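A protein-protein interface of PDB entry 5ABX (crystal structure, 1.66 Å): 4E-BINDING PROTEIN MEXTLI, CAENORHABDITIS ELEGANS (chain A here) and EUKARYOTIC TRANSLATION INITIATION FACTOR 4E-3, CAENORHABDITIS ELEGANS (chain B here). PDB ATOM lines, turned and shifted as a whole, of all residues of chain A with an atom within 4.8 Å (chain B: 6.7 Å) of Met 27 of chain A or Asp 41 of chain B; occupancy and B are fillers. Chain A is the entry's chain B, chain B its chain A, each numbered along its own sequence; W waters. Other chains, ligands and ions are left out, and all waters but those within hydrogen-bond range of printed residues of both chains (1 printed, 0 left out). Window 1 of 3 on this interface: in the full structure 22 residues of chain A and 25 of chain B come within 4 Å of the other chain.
The side-chain hydroxyl (OG) of Ser 34 of chain B lies within hydrogen-bond range of the side-chain carboxylate (OE1) of Glu 30 of chain A, 3.0 Å away. SD of Met 27 of chain A is in hydrogen-bond range of N of Leu 45 of chain B (3.7 Å).
Of the printed residues of chain B, Pro 24 of chain A touches Asp 41 and Ser 44. Printed residues of chain B within 4 Å of Glu 30 of chain A: Val 33 and Ser 34. Of the printed residues of chain B, Ile 31 of chain A touches Val 33 and Leu 45. Asp 41 of chain B touches just these residues of chain A: Pro 24 (3.6 Å) and Met 27 (3.6 Å). The nearest printed residue of chain B that does not touch Met 27 of chain A is Ser 44 of chain B (4.1 Å). The nearest printed residue of chain A that does not touch Asp 41 of chain B is Ile 23 of chain A (6.9 Å).
Of the 16 printed residues of chain B, 6 touch a printed residue of chain A. Hydrophobic or aromatic side chains of chain B within 4 Å of the printed part of chain A: Val 33, Leu 45 and His 48. Along chain B the printed residues that touch a printed residue of chain A span positions 33 to 48. Hydrophobic or aromatic side chains of chain A within 4 Å of the printed part of chain B: Ile 23, Pro 24, Met 27 and Ile 31. Among the printed residues, 11 pairs touch across the chains. Among the printed residues, no Asp or Glu carboxylate lies within 4 Å of a Lys or Arg side-chain nitrogen of the other chain.
The side-chain hydroxyl (OG1) of Thr 38 of chain B lies within hydrogen-bond range of the backbone NH (N) of Asp 41 of chain B (3.0 Å). OG of Ser 44 of chain B lies within hydrogen-bond range of O of Glu 40 of chain B, 3.2 Å away. O of Ser 44 of chain B sits at hydrogen-bond distance from ND1 of His 48 of chain B (2.8 Å).
Ile 23 of chain A touches Ser 44 of chain B. ND1 of His 48 of chain B touches CG2 of Ile 23 of chain A (2.9 Å). Pro 24 of chain A touches Asp 41 of chain B. Ser 44 of chain B touches Pro 24 of chain A. Met 27 of chain A touches Ser 34 of chain B (CG to OG, 3.996 Å). CE of Met 27 of chain A touches O of Asp 41 of chain B, 3.6 Å away. Glu 30 of chain A touches Val 33 of chain B. CG1 of Ile 31 of chain A touches CG1 of Val 33 of chain B, at 3.8 Å. Ile 31 of chain A touches Leu 45 of chain B.
Water W1 lies within hydrogen-bond range of the side-chain carboxylate of Glu 30 of chain A (2.8 Å) and the backbone NH of Leu 35 of chain B (2.9 Å).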
ATOM      1  N   ILE A  23       1.934  21.538  23.428  1.00  0.00           N
ATOM      2  CA  ILE A  23       3.195  22.243  23.609  1.00  0.00           C
ATOM      3  C   ILE A  23       4.181  21.287  24.240  1.00  0.00           C
ATOM      4  O   ILE A  23       3.777  20.260  24.796  1.00  0.00           O
ATOM      5  CB  ILE A  23       3.027  23.499  24.465  1.00  0.00           C
ATOM      6  CG1 ILE A  23       2.529  23.152  25.869  1.00  0.00           C
ATOM      7  CG2 ILE A  23       2.058  24.425  23.782  1.00  0.00           C
ATOM      8  CD1 ILE A  23       2.500  24.351  26.804  1.00  0.00           C
ATOM      9  N   PRO A  24       5.477  21.599  24.135  1.00  0.00           N
ATOM     10  CA  PRO A  24       6.479  20.738  24.768  1.00  0.00           C
ATOM     11  C   PRO A  24       6.203  20.624  26.260  1.00  0.00           C
ATOM     12  O   PRO A  24       5.838  21.619  26.889  1.00  0.00           O
ATOM     13  CB  PRO A  24       7.803  21.457  24.480  1.00  0.00           C
ATOM     14  CG  PRO A  24       7.529  22.278  23.266  1.00  0.00           C
ATOM     15  CD  PRO A  24       6.096  22.704  23.378  1.00  0.00           C
ATOM     16  N   ASP A  25       6.349  19.426  26.819  1.00  0.00           N
ATOM     17  CA  ASP A  25       5.967  19.213  28.206  1.00  0.00           C
ATOM     18  C   ASP A  25       6.777  20.104  29.145  1.00  0.00           C
ATOM     19  O   ASP A  25       6.258  20.548  30.161  1.00  0.00           O
ATOM     20  CB  ASP A  25       6.127  17.738  28.600  1.00  0.00           C
ATOM     21  CG  ASP A  25       5.308  17.374  29.826  1.00  0.00           C
ATOM     22  OD1 ASP A  25       4.062  17.463  29.762  1.00  0.00           O
ATOM     23  OD2 ASP A  25       5.898  17.006  30.865  1.00  0.00           O
ATOM     24  N   GLU A  26       8.035  20.373  28.805  1.00  0.00           N
ATOM     25  CA  GLU A  26       8.878  21.212  29.653  1.00  0.00           C
ATOM     26  C   GLU A  26       8.300  22.621  29.750  1.00  0.00           C
ATOM     27  O   GLU A  26       8.334  23.248  30.803  1.00  0.00           O
ATOM     28  CB  GLU A  26      10.305  21.275  29.113  1.00  0.00           C
ATOM     29  CG  GLU A  26      11.065  19.944  29.186  1.00  0.00           C
ATOM     30  CD  GLU A  26      10.646  18.933  28.118  1.00  0.00           C
ATOM     31  OE1 GLU A  26       9.967  19.317  27.134  1.00  0.00           O
ATOM     32  OE2 GLU A  26      11.015  17.745  28.265  1.00  0.00           O
ATOM     33  N   MET A  27       7.770  23.107  28.637  1.00  0.00           N
ATOM     34  CA  MET A  27       7.144  24.428  28.581  1.00  0.00           C
ATOM     35  C   MET A  27       5.854  24.474  29.412  1.00  0.00           C
ATOM     36  O   MET A  27       5.625  25.409  30.186  1.00  0.00           O
ATOM     37  CB  MET A  27       6.865  24.794  27.123  1.00  0.00           C
ATOM     38  CG  MET A  27       6.248  26.162  26.919  1.00  0.00           C
ATOM     39  SD  MET A  27       5.946  26.527  25.176  1.00  0.00           S
ATOM     40  CE  MET A  27       7.612  26.726  24.575  1.00  0.00           C
ATOM     41  N   LEU A  28       5.032  23.441  29.265  1.00  0.00           N
ATOM     42  CA  LEU A  28       3.816  23.293  30.052  1.00  0.00           C
ATOM     43  C   LEU A  28       4.136  23.330  31.545  1.00  0.00           C
ATOM     44  O   LEU A  28       3.459  24.003  32.318  1.00  0.00           O
ATOM     45  CB  LEU A  28       3.112  21.974  29.701  1.00  0.00           C
ATOM     46  CG  LEU A  28       1.802  21.662  30.425  1.00  0.00           C
ATOM     47  CD1 LEU A  28       0.698  22.560  29.943  1.00  0.00           C
ATOM     48  CD2 LEU A  28       1.420  20.202  30.209  1.00  0.00           C
ATOM     49  N   GLN A  29       5.169  22.590  31.939  1.00  0.00           N
ATOM     50  CA  GLN A  29       5.581  22.518  33.343  1.00  0.00           C
ATOM     51  C   GLN A  29       5.954  23.893  33.875  1.00  0.00           C
ATOM     52  O   GLN A  29       5.542  24.293  34.967  1.00  0.00           O
ATOM     53  CB  GLN A  29       6.775  21.584  33.520  1.00  0.00           C
ATOM     54  CG  GLN A  29       6.496  20.109  33.275  1.00  0.00           C
ATOM     55  CD  GLN A  29       7.779  19.305  33.202  1.00  0.00           C
ATOM     56  OE1 GLN A  29       8.779  19.680  33.808  1.00  0.00           O
ATOM     57  NE2 GLN A  29       7.767  18.215  32.438  1.00  0.00           N
ATOM     58  N   GLU A  30       6.732  24.615  33.079  1.00  0.00           N
ATOM     59  CA  GLU A  30       7.255  25.908  33.500  1.00  0.00           C
ATOM     60  C   GLU A  30       6.138  26.923  33.644  1.00  0.00           C
ATOM     61  O   GLU A  30       6.077  27.640  34.644  1.00  0.00           O
ATOM     62  CB  GLU A  30       8.316  26.401  32.507  1.00  0.00           C
ATOM     63  CG  GLU A  30       9.614  25.598  32.569  1.00  0.00           C
ATOM     64  CD  GLU A  30      10.520  25.787  31.353  1.00  0.00           C
ATOM     65  OE1 GLU A  30      10.170  26.568  30.440  1.00  0.00           O
ATOM     66  OE2 GLU A  30      11.588  25.138  31.312  1.00  0.00           O
ATOM     67  N   ILE A  31       5.238  26.979  32.668  1.00  0.00           N
ATOM     68  CA  ILE A  31       4.159  27.959  32.718  1.00  0.00           C
ATOM     69  C   ILE A  31       3.231  27.641  33.885  1.00  0.00           C
ATOM     70  O   ILE A  31       2.842  28.526  34.631  1.00  0.00           O
ATOM     71  CB  ILE A  31       3.347  27.993  31.421  1.00  0.00           C
ATOM     72  CG1 ILE A  31       4.243  28.338  30.234  1.00  0.00           C
ATOM     73  CG2 ILE A  31       2.224  29.037  31.515  1.00  0.00           C
ATOM     74  CD1 ILE A  31       3.598  28.080  28.900  1.00  0.00           C
ATOM     75  N   HIS B   7      13.437  25.430  13.280  1.00  0.00           N
ATOM     76  CA  HIS B   7      13.918  26.700  12.769  1.00  0.00           C
ATOM     77  C   HIS B   7      14.505  27.537  13.898  1.00  0.00           C
ATOM     78  O   HIS B   7      13.770  28.200  14.620  1.00  0.00           O
ATOM     79  CB  HIS B   7      12.783  27.464  12.089  1.00  0.00           C
ATOM     80  CG  HIS B   7      12.325  26.834  10.811  1.00  0.00           C
ATOM     81  ND1 HIS B   7      11.630  25.644  10.775  1.00  0.00           N
ATOM     82  CD2 HIS B   7      12.485  27.216   9.522  1.00  0.00           C
ATOM     83  CE1 HIS B   7      11.374  25.324   9.519  1.00  0.00           C
ATOM     84  NE2 HIS B   7      11.882  26.262   8.739  1.00  0.00           N
ATOM     85  N   VAL B  33       8.954  33.215  32.934  1.00  0.00           N
ATOM     86  CA  VAL B  33       8.052  32.110  32.658  1.00  0.00           C
ATOM     87  C   VAL B  33       8.737  31.009  31.846  1.00  0.00           C
ATOM     88  O   VAL B  33       8.831  29.869  32.298  1.00  0.00           O
ATOM     89  CB  VAL B  33       6.792  32.599  31.926  1.00  0.00           C
ATOM     90  CG1 VAL B  33       5.867  31.454  31.623  1.00  0.00           C
ATOM     91  CG2 VAL B  33       6.053  33.634  32.779  1.00  0.00           C
ATOM     92  N   SER B  34       9.216  31.344  30.655  1.00  0.00           N
ATOM     93  CA  SER B  34       9.784  30.333  29.776  1.00  0.00           C
ATOM     94  C   SER B  34      10.753  30.962  28.789  1.00  0.00           C
ATOM     95  O   SER B  34      10.594  32.114  28.394  1.00  0.00           O
ATOM     96  CB  SER B  34       8.669  29.587  29.035  1.00  0.00           C
ATOM     97  OG  SER B  34       9.186  28.492  28.301  1.00  0.00           O
ATOM     98  N   LEU B  35      11.789  30.205  28.437  1.00  0.00           N
ATOM     99  CA  LEU B  35      12.724  30.598  27.391  1.00  0.00           C
ATOM    100  C   LEU B  35      12.467  29.775  26.139  1.00  0.00           C
ATOM    101  O   LEU B  35      12.027  28.628  26.226  1.00  0.00           O
ATOM    102  CB  LEU B  35      14.171  30.403  27.841  1.00  0.00           C
ATOM    103  CG  LEU B  35      14.626  31.343  28.947  1.00  0.00           C
ATOM    104  CD1 LEU B  35      15.061  30.538  30.156  1.00  0.00           C
ATOM    105  CD2 LEU B  35      15.751  32.252  28.456  1.00  0.00           C
ATOM    106  N   PHE B  36      12.765  30.348  24.978  1.00  0.00           N
ATOM    107  CA  PHE B  36      12.636  29.629  23.712  1.00  0.00           C
ATOM    108  C   PHE B  36      13.649  30.175  22.724  1.00  0.00           C
ATOM    109  O   PHE B  36      14.117  31.308  22.853  1.00  0.00           O
ATOM    110  CB  PHE B  36      11.215  29.744  23.138  1.00  0.00           C
ATOM    111  CG  PHE B  36      10.792  31.148  22.832  1.00  0.00           C
ATOM    112  CD1 PHE B  36      11.034  31.715  21.593  1.00  0.00           C
ATOM    113  CD2 PHE B  36      10.153  31.914  23.792  1.00  0.00           C
ATOM    114  CE1 PHE B  36      10.647  33.019  21.327  1.00  0.00           C
ATOM    115  CE2 PHE B  36       9.760  33.213  23.522  1.00  0.00           C
ATOM    116  CZ  PHE B  36      10.007  33.763  22.295  1.00  0.00           C
ATOM    117  N   ASP B  37      14.008  29.364  21.740  1.00  0.00           N
ATOM    118  CA  ASP B  37      14.982  29.807  20.758  1.00  0.00           C
ATOM    119  C   ASP B  37      14.755  29.159  19.398  1.00  0.00           C
ATOM    120  O   ASP B  37      15.674  29.069  18.589  1.00  0.00           O
ATOM    121  CB  ASP B  37      16.415  29.559  21.265  1.00  0.00           C
ATOM    122  CG  ASP B  37      16.749  28.095  21.455  1.00  0.00           C
ATOM    123  OD1 ASP B  37      15.967  27.207  21.071  1.00  0.00           O
ATOM    124  OD2 ASP B  37      17.843  27.847  21.996  1.00  0.00           O
ATOM    125  N   THR B  38      13.503  28.782  19.128  1.00  0.00           N
ATOM    126  CA  THR B  38      13.094  28.329  17.801  1.00  0.00           C
ATOM    127  C   THR B  38      11.759  28.936  17.454  1.00  0.00           C
ATOM    128  O   THR B  38      11.009  29.349  18.340  1.00  0.00           O
ATOM    129  CB  THR B  38      12.950  26.799  17.694  1.00  0.00           C
ATOM    130  OG1 THR B  38      11.871  26.351  18.528  1.00  0.00           O
ATOM    131  CG2 THR B  38      14.227  26.096  18.102  1.00  0.00           C
ATOM    132  N   VAL B  39      11.470  28.976  16.162  1.00  0.00           N
ATOM    133  CA  VAL B  39      10.186  29.461  15.680  1.00  0.00           C
ATOM    134  C   VAL B  39       9.064  28.576  16.213  1.00  0.00           C
ATOM    135  O   VAL B  39       8.022  29.072  16.632  1.00  0.00           O
ATOM    136  CB  VAL B  39      10.149  29.496  14.145  1.00  0.00           C
ATOM    137  CG1 VAL B  39       8.758  29.850  13.631  1.00  0.00           C
ATOM    138  CG2 VAL B  39      11.168  30.493  13.624  1.00  0.00           C
ATOM    139  N   GLU B  40       9.290  27.265  16.199  1.00  0.00           N
ATOM    140  CA  GLU B  40       8.276  26.317  16.634  1.00  0.00           C
ATOM    141  C   GLU B  40       7.912  26.570  18.097  1.00  0.00           C
ATOM    142  O   GLU B  40       6.723  26.595  18.456  1.00  0.00           O
ATOM    143  CB  GLU B  40       8.768  24.881  16.421  1.00  0.00           C
ATOM    144  CG  GLU B  40       8.876  24.480  14.942  1.00  0.00           C
ATOM    145  CD  GLU B  40      10.085  25.075  14.212  1.00  0.00           C
ATOM    146  OE1 GLU B  40      11.079  25.483  14.861  1.00  0.00           O
ATOM    147  OE2 GLU B  40      10.037  25.126  12.963  1.00  0.00           O
ATOM    148  N   ASP B  41       8.920  26.790  18.939  1.00  0.00           N
ATOM    149  CA  ASP B  41       8.648  27.004  20.357  1.00  0.00           C
ATOM    150  C   ASP B  41       8.056  28.401  20.594  1.00  0.00           C
ATOM    151  O   ASP B  41       7.242  28.575  21.496  1.00  0.00           O
ATOM    152  CB  ASP B  41       9.902  26.808  21.211  1.00  0.00           C
ATOM    153  CG  ASP B  41      10.253  25.341  21.426  1.00  0.00           C
ATOM    154  OD1 ASP B  41       9.449  24.451  21.074  1.00  0.00           O
ATOM    155  OD2 ASP B  41      11.339  25.085  21.978  1.00  0.00           O
ATOM    156  N   PHE B  42       8.453  29.384  19.787  1.00  0.00           N
ATOM    157  CA  PHE B  42       7.824  30.706  19.848  1.00  0.00           C
ATOM    158  C   PHE B  42       6.307  30.590  19.668  1.00  0.00           C
ATOM    159  O   PHE B  42       5.544  31.124  20.465  1.00  0.00           O
ATOM    160  CB  PHE B  42       8.390  31.646  18.783  1.00  0.00           C
ATOM    161  CG  PHE B  42       7.562  32.898  18.576  1.00  0.00           C
ATOM    162  CD1 PHE B  42       7.527  33.876  19.545  1.00  0.00           C
ATOM    163  CD2 PHE B  42       6.820  33.085  17.418  1.00  0.00           C
ATOM    164  CE1 PHE B  42       6.771  35.032  19.370  1.00  0.00           C
ATOM    165  CE2 PHE B  42       6.067  34.236  17.235  1.00  0.00           C
ATOM    166  CZ  PHE B  42       6.041  35.204  18.206  1.00  0.00           C
ATOM    167  N   TRP B  43       5.877  29.896  18.616  1.00  0.00           N
ATOM    168  CA  TRP B  43       4.448  29.768  18.359  1.00  0.00           C
ATOM    169  C   TRP B  43       3.752  28.863  19.382  1.00  0.00           C
ATOM    170  O   TRP B  43       2.618  29.143  19.779  1.00  0.00           O
ATOM    171  CB  TRP B  43       4.193  29.250  16.940  1.00  0.00           C
ATOM    172  CG  TRP B  43       4.390  30.298  15.875  1.00  0.00           C
ATOM    173  CD1 TRP B  43       5.225  30.219  14.803  1.00  0.00           C
ATOM    174  CD2 TRP B  43       3.732  31.570  15.779  1.00  0.00           C
ATOM    175  NE1 TRP B  43       5.136  31.366  14.047  1.00  0.00           N
ATOM    176  CE2 TRP B  43       4.220  32.206  14.620  1.00  0.00           C
ATOM    177  CE3 TRP B  43       2.768  32.226  16.550  1.00  0.00           C
ATOM    178  CZ2 TRP B  43       3.789  33.469  14.221  1.00  0.00           C
ATOM    179  CZ3 TRP B  43       2.337  33.479  16.154  1.00  0.00           C
ATOM    180  CH2 TRP B  43       2.851  34.091  15.001  1.00  0.00           C
ATOM    181  N   SER B  44       4.413  27.796  19.820  1.00  0.00           N
ATOM    182  CA  SER B  44       3.839  26.960  20.877  1.00  0.00           C
ATOM    183  C   SER B  44       3.512  27.775  22.120  1.00  0.00           C
ATOM    184  O   SER B  44       2.430  27.641  22.698  1.00  0.00           O
ATOM    185  CB  SER B  44       4.787  25.824  21.254  1.00  0.00           C
ATOM    186  OG  SER B  44       4.756  24.817  20.280  1.00  0.00           O
ATOM    187  N   LEU B  45       4.445  28.633  22.522  1.00  0.00           N
ATOM    188  CA  LEU B  45       4.252  29.486  23.684  1.00  0.00           C
ATOM    189  C   LEU B  45       3.154  30.512  23.438  1.00  0.00           C
ATOM    190  O   LEU B  45       2.215  30.619  24.231  1.00  0.00           O
ATOM    191  CB  LEU B  45       5.563  30.185  24.048  1.00  0.00           C
ATOM    192  CG  LEU B  45       5.523  31.145  25.235  1.00  0.00           C
ATOM    193  CD1 LEU B  45       5.142  30.393  26.506  1.00  0.00           C
ATOM    194  CD2 LEU B  45       6.857  31.814  25.410  1.00  0.00           C
ATOM    195  N   TYR B  46       3.264  31.255  22.338  1.00  0.00           N
ATOM    196  CA  TYR B  46       2.296  32.301  22.049  1.00  0.00           C
ATOM    197  C   TYR B  46       0.883  31.728  21.942  1.00  0.00           C
ATOM    198  O   TYR B  46      -0.075  32.331  22.441  1.00  0.00           O
ATOM    199  CB  TYR B  46       2.645  33.047  20.755  1.00  0.00           C
ATOM    200  CG  TYR B  46       1.710  34.200  20.543  1.00  0.00           C
ATOM    201  CD1 TYR B  46       1.915  35.396  21.205  1.00  0.00           C
ATOM    202  CD2 TYR B  46       0.597  34.074  19.734  1.00  0.00           C
ATOM    203  CE1 TYR B  46       1.048  36.459  21.049  1.00  0.00           C
ATOM    204  CE2 TYR B  46      -0.285  35.136  19.566  1.00  0.00           C
ATOM    205  CZ  TYR B  46      -0.052  36.318  20.231  1.00  0.00           C
ATOM    206  OH  TYR B  46      -0.910  37.382  20.088  1.00  0.00           O
ATOM    207  N   HIS B  48      -0.458  29.246  23.392  1.00  0.00           N
ATOM    208  CA  HIS B  48      -0.976  28.611  24.601  1.00  0.00           C
ATOM    209  C   HIS B  48      -0.848  29.479  25.854  1.00  0.00           C
ATOM    210  O   HIS B  48      -0.850  28.965  26.979  1.00  0.00           O
ATOM    211  CB  HIS B  48      -0.280  27.269  24.802  1.00  0.00           C
ATOM    212  CG  HIS B  48      -0.619  26.273  23.737  1.00  0.00           C
ATOM    213  ND1 HIS B  48       0.097  26.162  22.565  1.00  0.00           N
ATOM    214  CD2 HIS B  48      -1.639  25.389  23.640  1.00  0.00           C
ATOM    215  CE1 HIS B  48      -0.447  25.229  21.805  1.00  0.00           C
ATOM    216  NE2 HIS B  48      -1.501  24.742  22.434  1.00  0.00           N
HETATM  217  O   HOH W   1      12.600  27.797  29.909  1.00  0.00           O
